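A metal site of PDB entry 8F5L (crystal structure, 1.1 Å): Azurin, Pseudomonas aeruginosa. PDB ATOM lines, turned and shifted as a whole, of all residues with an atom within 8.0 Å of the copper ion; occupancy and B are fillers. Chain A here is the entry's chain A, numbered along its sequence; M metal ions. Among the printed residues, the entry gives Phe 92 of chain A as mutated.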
ATOM      1  N   GLY A  29     -31.518  -7.827  -5.410  1.00  0.00           N
ATOM      2  CA  GLY A  29     -30.392  -8.719  -5.178  1.00  0.00           C
ATOM      3  C   GLY A  29     -30.182  -8.866  -3.681  1.00  0.00           C
ATOM      4  O   GLY A  29     -30.214  -7.863  -2.977  1.00  0.00           O
ATOM      5  N   ASN A  30     -30.000 -10.068  -3.180  1.00  0.00           N
ATOM      6  CA  ASN A  30     -30.073 -10.348  -1.746  1.00  0.00           C
ATOM      7  C   ASN A  30     -28.698 -10.711  -1.183  1.00  0.00           C
ATOM      8  O   ASN A  30     -27.666 -10.585  -1.853  1.00  0.00           O
ATOM      9  CB  ASN A  30     -31.138 -11.413  -1.466  1.00  0.00           C
ATOM     10  CG  ASN A  30     -30.763 -12.758  -2.000  1.00  0.00           C
ATOM     11  OD1 ASN A  30     -29.656 -12.988  -2.447  1.00  0.00           O
ATOM     12  ND2 ASN A  30     -31.708 -13.697  -1.942  1.00  0.00           N
ATOM     13  N   MET A  33     -26.588 -13.694  -2.939  1.00  0.00           N
ATOM     14  CA  MET A  33     -26.009 -13.637  -4.262  1.00  0.00           C
ATOM     15  C   MET A  33     -27.002 -14.095  -5.324  1.00  0.00           C
ATOM     16  O   MET A  33     -26.638 -14.763  -6.280  1.00  0.00           O
ATOM     17  CB  MET A  33     -24.721 -14.451  -4.331  1.00  0.00           C
ATOM     18  CG  MET A  33     -23.772 -13.912  -5.347  1.00  0.00           C
ATOM     19  SD  MET A  33     -22.134 -14.840  -5.396  1.00  0.00           S
ATOM     20  CE  MET A  33     -22.612 -16.373  -6.166  1.00  0.00           C
ATOM     21  N   GLN A  34     -28.250 -13.687  -5.166  1.00  0.00           N
ATOM     22  CA  GLN A  34     -29.302 -14.015  -6.114  1.00  0.00           C
ATOM     23  C   GLN A  34     -30.090 -12.785  -6.487  1.00  0.00           C
ATOM     24  O   GLN A  34     -30.388 -11.944  -5.633  1.00  0.00           O
ATOM     25  CB  GLN A  34     -30.291 -15.021  -5.523  1.00  0.00           C
ATOM     26  CG  GLN A  34     -29.696 -16.303  -5.052  1.00  0.00           C
ATOM     27  CD  GLN A  34     -30.673 -17.079  -4.189  1.00  0.00           C
ATOM     28  OE1 GLN A  34     -31.296 -16.513  -3.276  1.00  0.00           O
ATOM     29  NE2 GLN A  34     -30.833 -18.369  -4.476  1.00  0.00           N
ATOM     30  N   PHE A  35     -30.468 -12.692  -7.757  1.00  0.00           N
ATOM     31  CA  PHE A  35     -31.550 -11.801  -8.160  1.00  0.00           C
ATOM     32  C   PHE A  35     -32.872 -12.509  -7.876  1.00  0.00           C
ATOM     33  O   PHE A  35     -32.957 -13.736  -7.903  1.00  0.00           O
ATOM     34  CB  PHE A  35     -31.516 -11.515  -9.675  1.00  0.00           C
ATOM     35  CG  PHE A  35     -30.442 -10.561 -10.138  1.00  0.00           C
ATOM     36  CD1 PHE A  35     -30.294  -9.311  -9.587  1.00  0.00           C
ATOM     37  CD2 PHE A  35     -29.625 -10.912 -11.195  1.00  0.00           C
ATOM     38  CE1 PHE A  35     -29.321  -8.429 -10.054  1.00  0.00           C
ATOM     39  CE2 PHE A  35     -28.664 -10.045 -11.673  1.00  0.00           C
ATOM     40  CZ  PHE A  35     -28.519  -8.802 -11.101  1.00  0.00           C
ATOM     41  N   LEU A  53     -33.525  -1.387  -9.124  1.00  0.00           N
ATOM     42  CA  LEU A  53     -32.788  -2.368  -8.354  1.00  0.00           C
ATOM     43  C   LEU A  53     -32.782  -1.971  -6.885  1.00  0.00           C
ATOM     44  O   LEU A  53     -32.596  -0.800  -6.561  1.00  0.00           O
ATOM     45  CB  LEU A  53     -31.344  -2.482  -8.871  1.00  0.00           C
ATOM     46  CG  LEU A  53     -30.502  -3.571  -8.218  1.00  0.00           C
ATOM     47  CD1 LEU A  53     -30.968  -4.965  -8.580  1.00  0.00           C
ATOM     48  CD2 LEU A  53     -29.030  -3.378  -8.586  1.00  0.00           C
ATOM     49  N   HIS A  55     -31.818  -3.786  -2.699  1.00  0.00           N
ATOM     50  CA  HIS A  55     -30.967  -4.750  -2.004  1.00  0.00           C
ATOM     51  C   HIS A  55     -31.564  -4.961  -0.625  1.00  0.00           C
ATOM     52  O   HIS A  55     -31.245  -4.236   0.318  1.00  0.00           O
ATOM     53  CB  HIS A  55     -29.542  -4.198  -1.890  1.00  0.00           C
ATOM     54  CG  HIS A  55     -28.530  -5.215  -1.464  1.00  0.00           C
ATOM     55  ND1 HIS A  55     -28.754  -6.148  -0.467  1.00  0.00           N
ATOM     56  CD2 HIS A  55     -27.261  -5.430  -1.902  1.00  0.00           C
ATOM     57  CE1 HIS A  55     -27.676  -6.897  -0.329  1.00  0.00           C
ATOM     58  NE2 HIS A  55     -26.757  -6.470  -1.182  1.00  0.00           N
ATOM     59  N   LYS A  61     -21.995  -3.022   0.389  1.00  0.00           N
ATOM     60  CA  LYS A  61     -21.669  -3.224  -1.010  1.00  0.00           C
ATOM     61  C   LYS A  61     -20.266  -3.792  -1.247  1.00  0.00           C
ATOM     62  O   LYS A  61     -20.052  -4.406  -2.301  1.00  0.00           O
ATOM     63  CB  LYS A  61     -21.901  -1.951  -1.818  1.00  0.00           C
ATOM     64  CG  LYS A  61     -20.877  -0.905  -1.672  1.00  0.00           C
ATOM     65  CD  LYS A  61     -21.244   0.283  -2.544  1.00  0.00           C
ATOM     66  CE  LYS A  61     -20.241   1.381  -2.416  1.00  0.00           C
ATOM     67  NZ  LYS A  61     -20.772   2.628  -3.026  1.00  0.00           N
ATOM     68  N   VAL A  63     -18.982  -6.262   0.456  1.00  0.00           N
ATOM     69  CA  VAL A  63     -19.103  -7.697   0.711  1.00  0.00           C
ATOM     70  C   VAL A  63     -20.066  -8.354  -0.264  1.00  0.00           C
ATOM     71  O   VAL A  63     -19.843  -9.496  -0.682  1.00  0.00           O
ATOM     72  CB  VAL A  63     -19.575  -7.921   2.162  1.00  0.00           C
ATOM     73  CG1 VAL A  63     -20.000  -9.360   2.404  1.00  0.00           C
ATOM     74  CG2 VAL A  63     -18.521  -7.533   3.163  1.00  0.00           C
ATOM     75  N   MET A  64     -21.169  -7.694  -0.586  1.00  0.00           N
ATOM     76  CA  MET A  64     -22.269  -8.304  -1.330  1.00  0.00           C
ATOM     77  C   MET A  64     -22.950  -7.196  -2.119  1.00  0.00           C
ATOM     78  O   MET A  64     -24.184  -7.094  -2.142  1.00  0.00           O
ATOM     79  CB  MET A  64     -23.227  -9.008  -0.366  1.00  0.00           C
ATOM     80  CG  MET A  64     -24.326  -9.821  -0.993  1.00  0.00           C
ATOM     81  SD  MET A  64     -23.850 -11.074  -2.198  1.00  0.00           S
ATOM     82  CE  MET A  64     -23.024 -12.302  -1.206  1.00  0.00           C
ATOM     83  N   GLY A  65     -22.170  -6.367  -2.801  1.00  0.00           N
ATOM     84  CA  GLY A  65     -22.769  -5.350  -3.646  1.00  0.00           C
ATOM     85  C   GLY A  65     -23.312  -5.964  -4.921  1.00  0.00           C
ATOM     86  O   GLY A  65     -22.799  -6.965  -5.403  1.00  0.00           O
ATOM     87  N   HIS A  66     -24.352  -5.345  -5.455  1.00  0.00           N
ATOM     88  CA  HIS A  66     -24.951  -5.793  -6.693  1.00  0.00           C
ATOM     89  C   HIS A  66     -25.191  -4.638  -7.646  1.00  0.00           C
ATOM     90  O   HIS A  66     -25.562  -3.543  -7.229  1.00  0.00           O
ATOM     91  CB  HIS A  66     -26.301  -6.448  -6.451  1.00  0.00           C
ATOM     92  CG  HIS A  66     -26.248  -7.617  -5.543  1.00  0.00           C
ATOM     93  ND1 HIS A  66     -25.405  -8.684  -5.754  1.00  0.00           N
ATOM     94  CD2 HIS A  66     -26.980  -7.898  -4.445  1.00  0.00           C
ATOM     95  CE1 HIS A  66     -25.597  -9.574  -4.791  1.00  0.00           C
ATOM     96  NE2 HIS A  66     -26.555  -9.129  -3.990  1.00  0.00           N
ATOM     97  N   ASN A  67     -25.021  -4.912  -8.917  1.00  0.00           N
ATOM     98  CA  ASN A  67     -25.525  -4.054  -9.963  1.00  0.00           C
ATOM     99  C   ASN A  67     -26.359  -4.897 -10.900  1.00  0.00           C
ATOM    100  O   ASN A  67     -26.465  -6.122 -10.758  1.00  0.00           O
ATOM    101  CB  ASN A  67     -24.389  -3.285 -10.673  1.00  0.00           C
ATOM    102  CG  ASN A  67     -23.306  -4.195 -11.237  1.00  0.00           C
ATOM    103  OD1 ASN A  67     -23.491  -5.374 -11.460  1.00  0.00           O
ATOM    104  ND2 ASN A  67     -22.157  -3.599 -11.521  1.00  0.00           N
ATOM    105  N   TRP A  68     -27.005  -4.207 -11.826  1.00  0.00           N
ATOM    106  CA  TRP A  68     -27.778  -4.841 -12.872  1.00  0.00           C
ATOM    107  C   TRP A  68     -27.212  -4.286 -14.166  1.00  0.00           C
ATOM    108  O   TRP A  68     -27.247  -3.070 -14.371  1.00  0.00           O
ATOM    109  CB  TRP A  68     -29.263  -4.531 -12.715  1.00  0.00           C
ATOM    110  CG  TRP A  68     -30.118  -5.232 -13.710  1.00  0.00           C
ATOM    111  CD1 TRP A  68     -30.726  -6.442 -13.553  1.00  0.00           C
ATOM    112  CD2 TRP A  68     -30.441  -4.787 -15.027  1.00  0.00           C
ATOM    113  NE1 TRP A  68     -31.432  -6.777 -14.682  1.00  0.00           N
ATOM    114  CE2 TRP A  68     -31.281  -5.778 -15.607  1.00  0.00           C
ATOM    115  CE3 TRP A  68     -30.132  -3.661 -15.786  1.00  0.00           C
ATOM    116  CZ2 TRP A  68     -31.789  -5.670 -16.892  1.00  0.00           C
ATOM    117  CZ3 TRP A  68     -30.656  -3.568 -17.068  1.00  0.00           C
ATOM    118  CH2 TRP A  68     -31.471  -4.567 -17.592  1.00  0.00           C
ATOM    119  N   PHE A  92     -17.046  -2.151 -10.455  1.00  0.00           N
ATOM    120  CA  PHE A  92     -16.779  -3.382 -11.192  1.00  0.00           C
ATOM    121  C   PHE A  92     -17.266  -3.306 -12.633  1.00  0.00           C
ATOM    122  O   PHE A  92     -17.743  -4.291 -13.209  1.00  0.00           O
ATOM    123  CB  PHE A  92     -17.344  -4.593 -10.474  1.00  0.00           C
ATOM    124  CG  PHE A  92     -16.648  -4.878  -9.180  1.00  0.00           C
ATOM    125  CD1 PHE A  92     -15.310  -5.221  -9.148  1.00  0.00           C
ATOM    126  CD2 PHE A  92     -17.330  -4.805  -7.978  1.00  0.00           C
ATOM    127  CE1 PHE A  92     -14.681  -5.506  -7.950  1.00  0.00           C
ATOM    128  CE2 PHE A  92     -16.704  -5.077  -6.795  1.00  0.00           C
ATOM    129  CZ  PHE A  92     -15.381  -5.421  -6.788  1.00  0.00           C
ATOM    130  N   LEU A 106     -23.609   0.050  -8.505  1.00  0.00           N
ATOM    131  CA  LEU A 106     -23.431  -1.032  -7.542  1.00  0.00           C
ATOM    132  C   LEU A 106     -24.005  -0.569  -6.214  1.00  0.00           C
ATOM    133  O   LEU A 106     -23.642   0.497  -5.706  1.00  0.00           O
ATOM    134  CB  LEU A 106     -21.940  -1.348  -7.394  1.00  0.00           C
ATOM    135  CG  LEU A 106     -21.611  -2.607  -6.591  1.00  0.00           C
ATOM    136  CD1 LEU A 106     -21.770  -3.824  -7.478  1.00  0.00           C
ATOM    137  CD2 LEU A 106     -20.202  -2.537  -6.012  1.00  0.00           C
ATOM    138  N   ILE A 107     -24.882  -1.381  -5.634  1.00  0.00           N
ATOM    139  CA  ILE A 107     -25.547  -1.014  -4.389  1.00  0.00           C
ATOM    140  C   ILE A 107     -25.322  -2.065  -3.313  1.00  0.00           C
ATOM    141  O   ILE A 107     -25.170  -3.253  -3.581  1.00  0.00           O
ATOM    142  CB  ILE A 107     -27.055  -0.780  -4.581  1.00  0.00           C
ATOM    143  CG1 ILE A 107     -27.768  -2.053  -5.112  1.00  0.00           C
ATOM    144  CG2 ILE A 107     -27.284   0.367  -5.516  1.00  0.00           C
ATOM    145  CD1 ILE A 107     -29.292  -1.939  -5.138  1.00  0.00           C
ATOM    146  N   PHE A 131     -26.918  -9.327 -15.846  1.00  0.00           N
ATOM    147  CA  PHE A 131     -25.994  -9.929 -14.881  1.00  0.00           C
ATOM    148  C   PHE A 131     -25.521  -8.861 -13.904  1.00  0.00           C
ATOM    149  O   PHE A 131     -25.638  -7.665 -14.151  1.00  0.00           O
ATOM    150  CB  PHE A 131     -24.791 -10.572 -15.582  1.00  0.00           C
ATOM    151  CG  PHE A 131     -24.181  -9.712 -16.651  1.00  0.00           C
ATOM    152  CD1 PHE A 131     -24.695  -9.708 -17.934  1.00  0.00           C
ATOM    153  CD2 PHE A 131     -23.098  -8.894 -16.383  1.00  0.00           C
ATOM    154  CE1 PHE A 131     -24.172  -8.929 -18.910  1.00  0.00           C
ATOM    155  CE2 PHE A 131     -22.549  -8.112 -17.375  1.00  0.00           C
ATOM    156  CZ  PHE A 131     -23.098  -8.139 -18.638  1.00  0.00           C
ATOM    157  N   CYS A 132     -24.984  -9.331 -12.799  1.00  0.00           N
ATOM    158  CA  CYS A 132     -24.226  -8.523 -11.852  1.00  0.00           C
ATOM    159  C   CYS A 132     -22.746  -8.749 -12.110  1.00  0.00           C
ATOM    160  O   CYS A 132     -22.330  -9.878 -12.322  1.00  0.00           O
ATOM    161  CB  CYS A 132     -24.554  -8.955 -10.426  1.00  0.00           C
ATOM    162  SG  CYS A 132     -23.593  -8.080  -9.145  1.00  0.00           S
ATOM    163  N   THR A 133     -21.970  -7.659 -12.108  1.00  0.00           N
ATOM    164  CA  THR A 133     -20.529  -7.769 -12.349  1.00  0.00           C
ATOM    165  C   THR A 133     -19.687  -7.776 -11.091  1.00  0.00           C
ATOM    166  O   THR A 133     -18.459  -7.805 -11.190  1.00  0.00           O
ATOM    167  CB  THR A 133     -20.020  -6.673 -13.295  1.00  0.00           C
ATOM    168  OG1 THR A 133     -20.214  -5.393 -12.677  1.00  0.00           O
ATOM    169  CG2 THR A 133     -20.708  -6.732 -14.628  1.00  0.00           C
ATOM    170  N   PHE A 134     -20.271  -7.776  -9.905  1.00  0.00           N
ATOM    171  CA  PHE A 134     -19.444  -7.992  -8.724  1.00  0.00           C
ATOM    172  C   PHE A 134     -18.764  -9.346  -8.904  1.00  0.00           C
ATOM    173  O   PHE A 134     -19.425 -10.316  -9.281  1.00  0.00           O
ATOM    174  CB  PHE A 134     -20.295  -8.002  -7.456  1.00  0.00           C
ATOM    175  CG  PHE A 134     -19.499  -7.991  -6.186  1.00  0.00           C
ATOM    176  CD1 PHE A 134     -18.781  -9.111  -5.797  1.00  0.00           C
ATOM    177  CD2 PHE A 134     -19.497  -6.885  -5.369  1.00  0.00           C
ATOM    178  CE1 PHE A 134     -18.048  -9.106  -4.629  1.00  0.00           C
ATOM    179  CE2 PHE A 134     -18.776  -6.884  -4.190  1.00  0.00           C
ATOM    180  CZ  PHE A 134     -18.042  -7.999  -3.826  1.00  0.00           C
ATOM    181  N   PRO A 135     -17.453  -9.438  -8.709  1.00  0.00           N
ATOM    182  CA  PRO A 135     -16.742 -10.662  -9.131  1.00  0.00           C
ATOM    183  C   PRO A 135     -17.314 -11.914  -8.488  1.00  0.00           C
ATOM    184  O   PRO A 135     -17.571 -11.960  -7.286  1.00  0.00           O
ATOM    185  CB  PRO A 135     -15.290 -10.412  -8.710  1.00  0.00           C
ATOM    186  CG  PRO A 135     -15.164  -8.922  -8.686  1.00  0.00           C
ATOM    187  CD  PRO A 135     -16.528  -8.358  -8.324  1.00  0.00           C
ATOM    188  N   GLY A 136     -17.505 -12.931  -9.325  1.00  0.00           N
ATOM    189  CA  GLY A 136     -18.083 -14.163  -8.923  1.00  0.00           C
ATOM    190  C   GLY A 136     -19.592 -14.209  -8.972  1.00  0.00           C
ATOM    191  O   GLY A 136     -20.169 -15.296  -9.131  1.00  0.00           O
ATOM    192  N   HIS A 137     -20.260 -13.065  -8.833  1.00  0.00           N
ATOM    193  CA  HIS A 137     -21.712 -13.096  -8.636  1.00  0.00           C
ATOM    194  C   HIS A 137     -22.450 -13.648  -9.846  1.00  0.00           C
ATOM    195  O   HIS A 137     -23.498 -14.274  -9.677  1.00  0.00           O
ATOM    196  CB  HIS A 137     -22.230 -11.701  -8.316  1.00  0.00           C
ATOM    197  CG  HIS A 137     -21.923 -11.270  -6.928  1.00  0.00           C
ATOM    198  ND1 HIS A 137     -22.616 -10.250  -6.313  1.00  0.00           N
ATOM    199  CD2 HIS A 137     -21.037 -11.745  -6.018  1.00  0.00           C
ATOM    200  CE1 HIS A 137     -22.136 -10.086  -5.090  1.00  0.00           C
ATOM    201  NE2 HIS A 137     -21.212 -11.004  -4.870  1.00  0.00           N
ATOM    202  N   SER A 138     -21.940 -13.418 -11.055  1.00  0.00           N
ATOM    203  CA  SER A 138     -22.651 -13.870 -12.248  1.00  0.00           C
ATOM    204  C   SER A 138     -22.742 -15.389 -12.359  1.00  0.00           C
ATOM    205  O   SER A 138     -23.487 -15.878 -13.212  1.00  0.00           O
ATOM    206  CB  SER A 138     -22.032 -13.279 -13.506  1.00  0.00           C
ATOM    207  OG  SER A 138     -20.737 -13.812 -13.745  1.00  0.00           O
ATOM    208  N   MET A 141     -26.046 -14.764 -10.632  1.00  0.00           N
ATOM    209  CA  MET A 141     -26.762 -13.527 -10.945  1.00  0.00           C
ATOM    210  C   MET A 141     -26.571 -13.234 -12.416  1.00  0.00           C
ATOM    211  O   MET A 141     -25.797 -12.371 -12.822  1.00  0.00           O
ATOM    212  CB  MET A 141     -26.286 -12.394 -10.059  1.00  0.00           C
ATOM    213  CG  MET A 141     -26.455 -12.725  -8.599  1.00  0.00           C
ATOM    214  SD  MET A 141     -26.061 -11.393  -7.464  1.00  0.00           S
ATOM    215  CE  MET A 141     -27.439 -10.264  -7.747  1.00  0.00           C
HETATM  216 CU    CU M   1     -23.999  -9.013  -7.202  1.00  0.00          CU
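Merely in contact with the copper ion: Gly 65 (3.0 Å), Phe 134 (3.8 Å) and Met 141 (3.2 Å). Of the 26 residues printed, 6 come within 4 Å of the copper ion. The nearest printed residue that does not touch the copper ion is Asn 67 (4.6 Å).
ND1 of His 66 lies close to SD of Met 141 (3.3 Å). A ring nitrogen (NE2) of His 66 lies close to the side-chain sulfur (SD) of Met 64 (3.8 Å). NE2 of His 66 sits at hydrogen-bond distance from O of Asn 30. The backbone carbonyl oxygen (O) of His 66 sits at hydrogen-bond distance from the backbone NH (N) of Ile 107, 2.8 Å away. The backbone carbonyl oxygen of Gly 65 sits close to a ring nitrogen (ND1) of His 137 (3.4 Å). A ring nitrogen (NE2) of His 137 lies close to the side-chain sulfur (SD) of Met 64 (3.8 Å). The backbone carbonyl oxygen (O) of Met 141 lies within hydrogen-bond range of the backbone NH (N) of Cys 132 (3.1 Å). The side-chain sulfur of Cys 132 lies close to the backbone NH of Asn 67, 3.5 Å away.
The copper ion is bound by a ring nitrogen (ND1) of His 66 (2.0 Å). A ring nitrogen (ND1) of His 137 is bound to the copper ion, 2.1 Å away. SG of Cys 132 is bound to the copper ion (2.2 Å).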
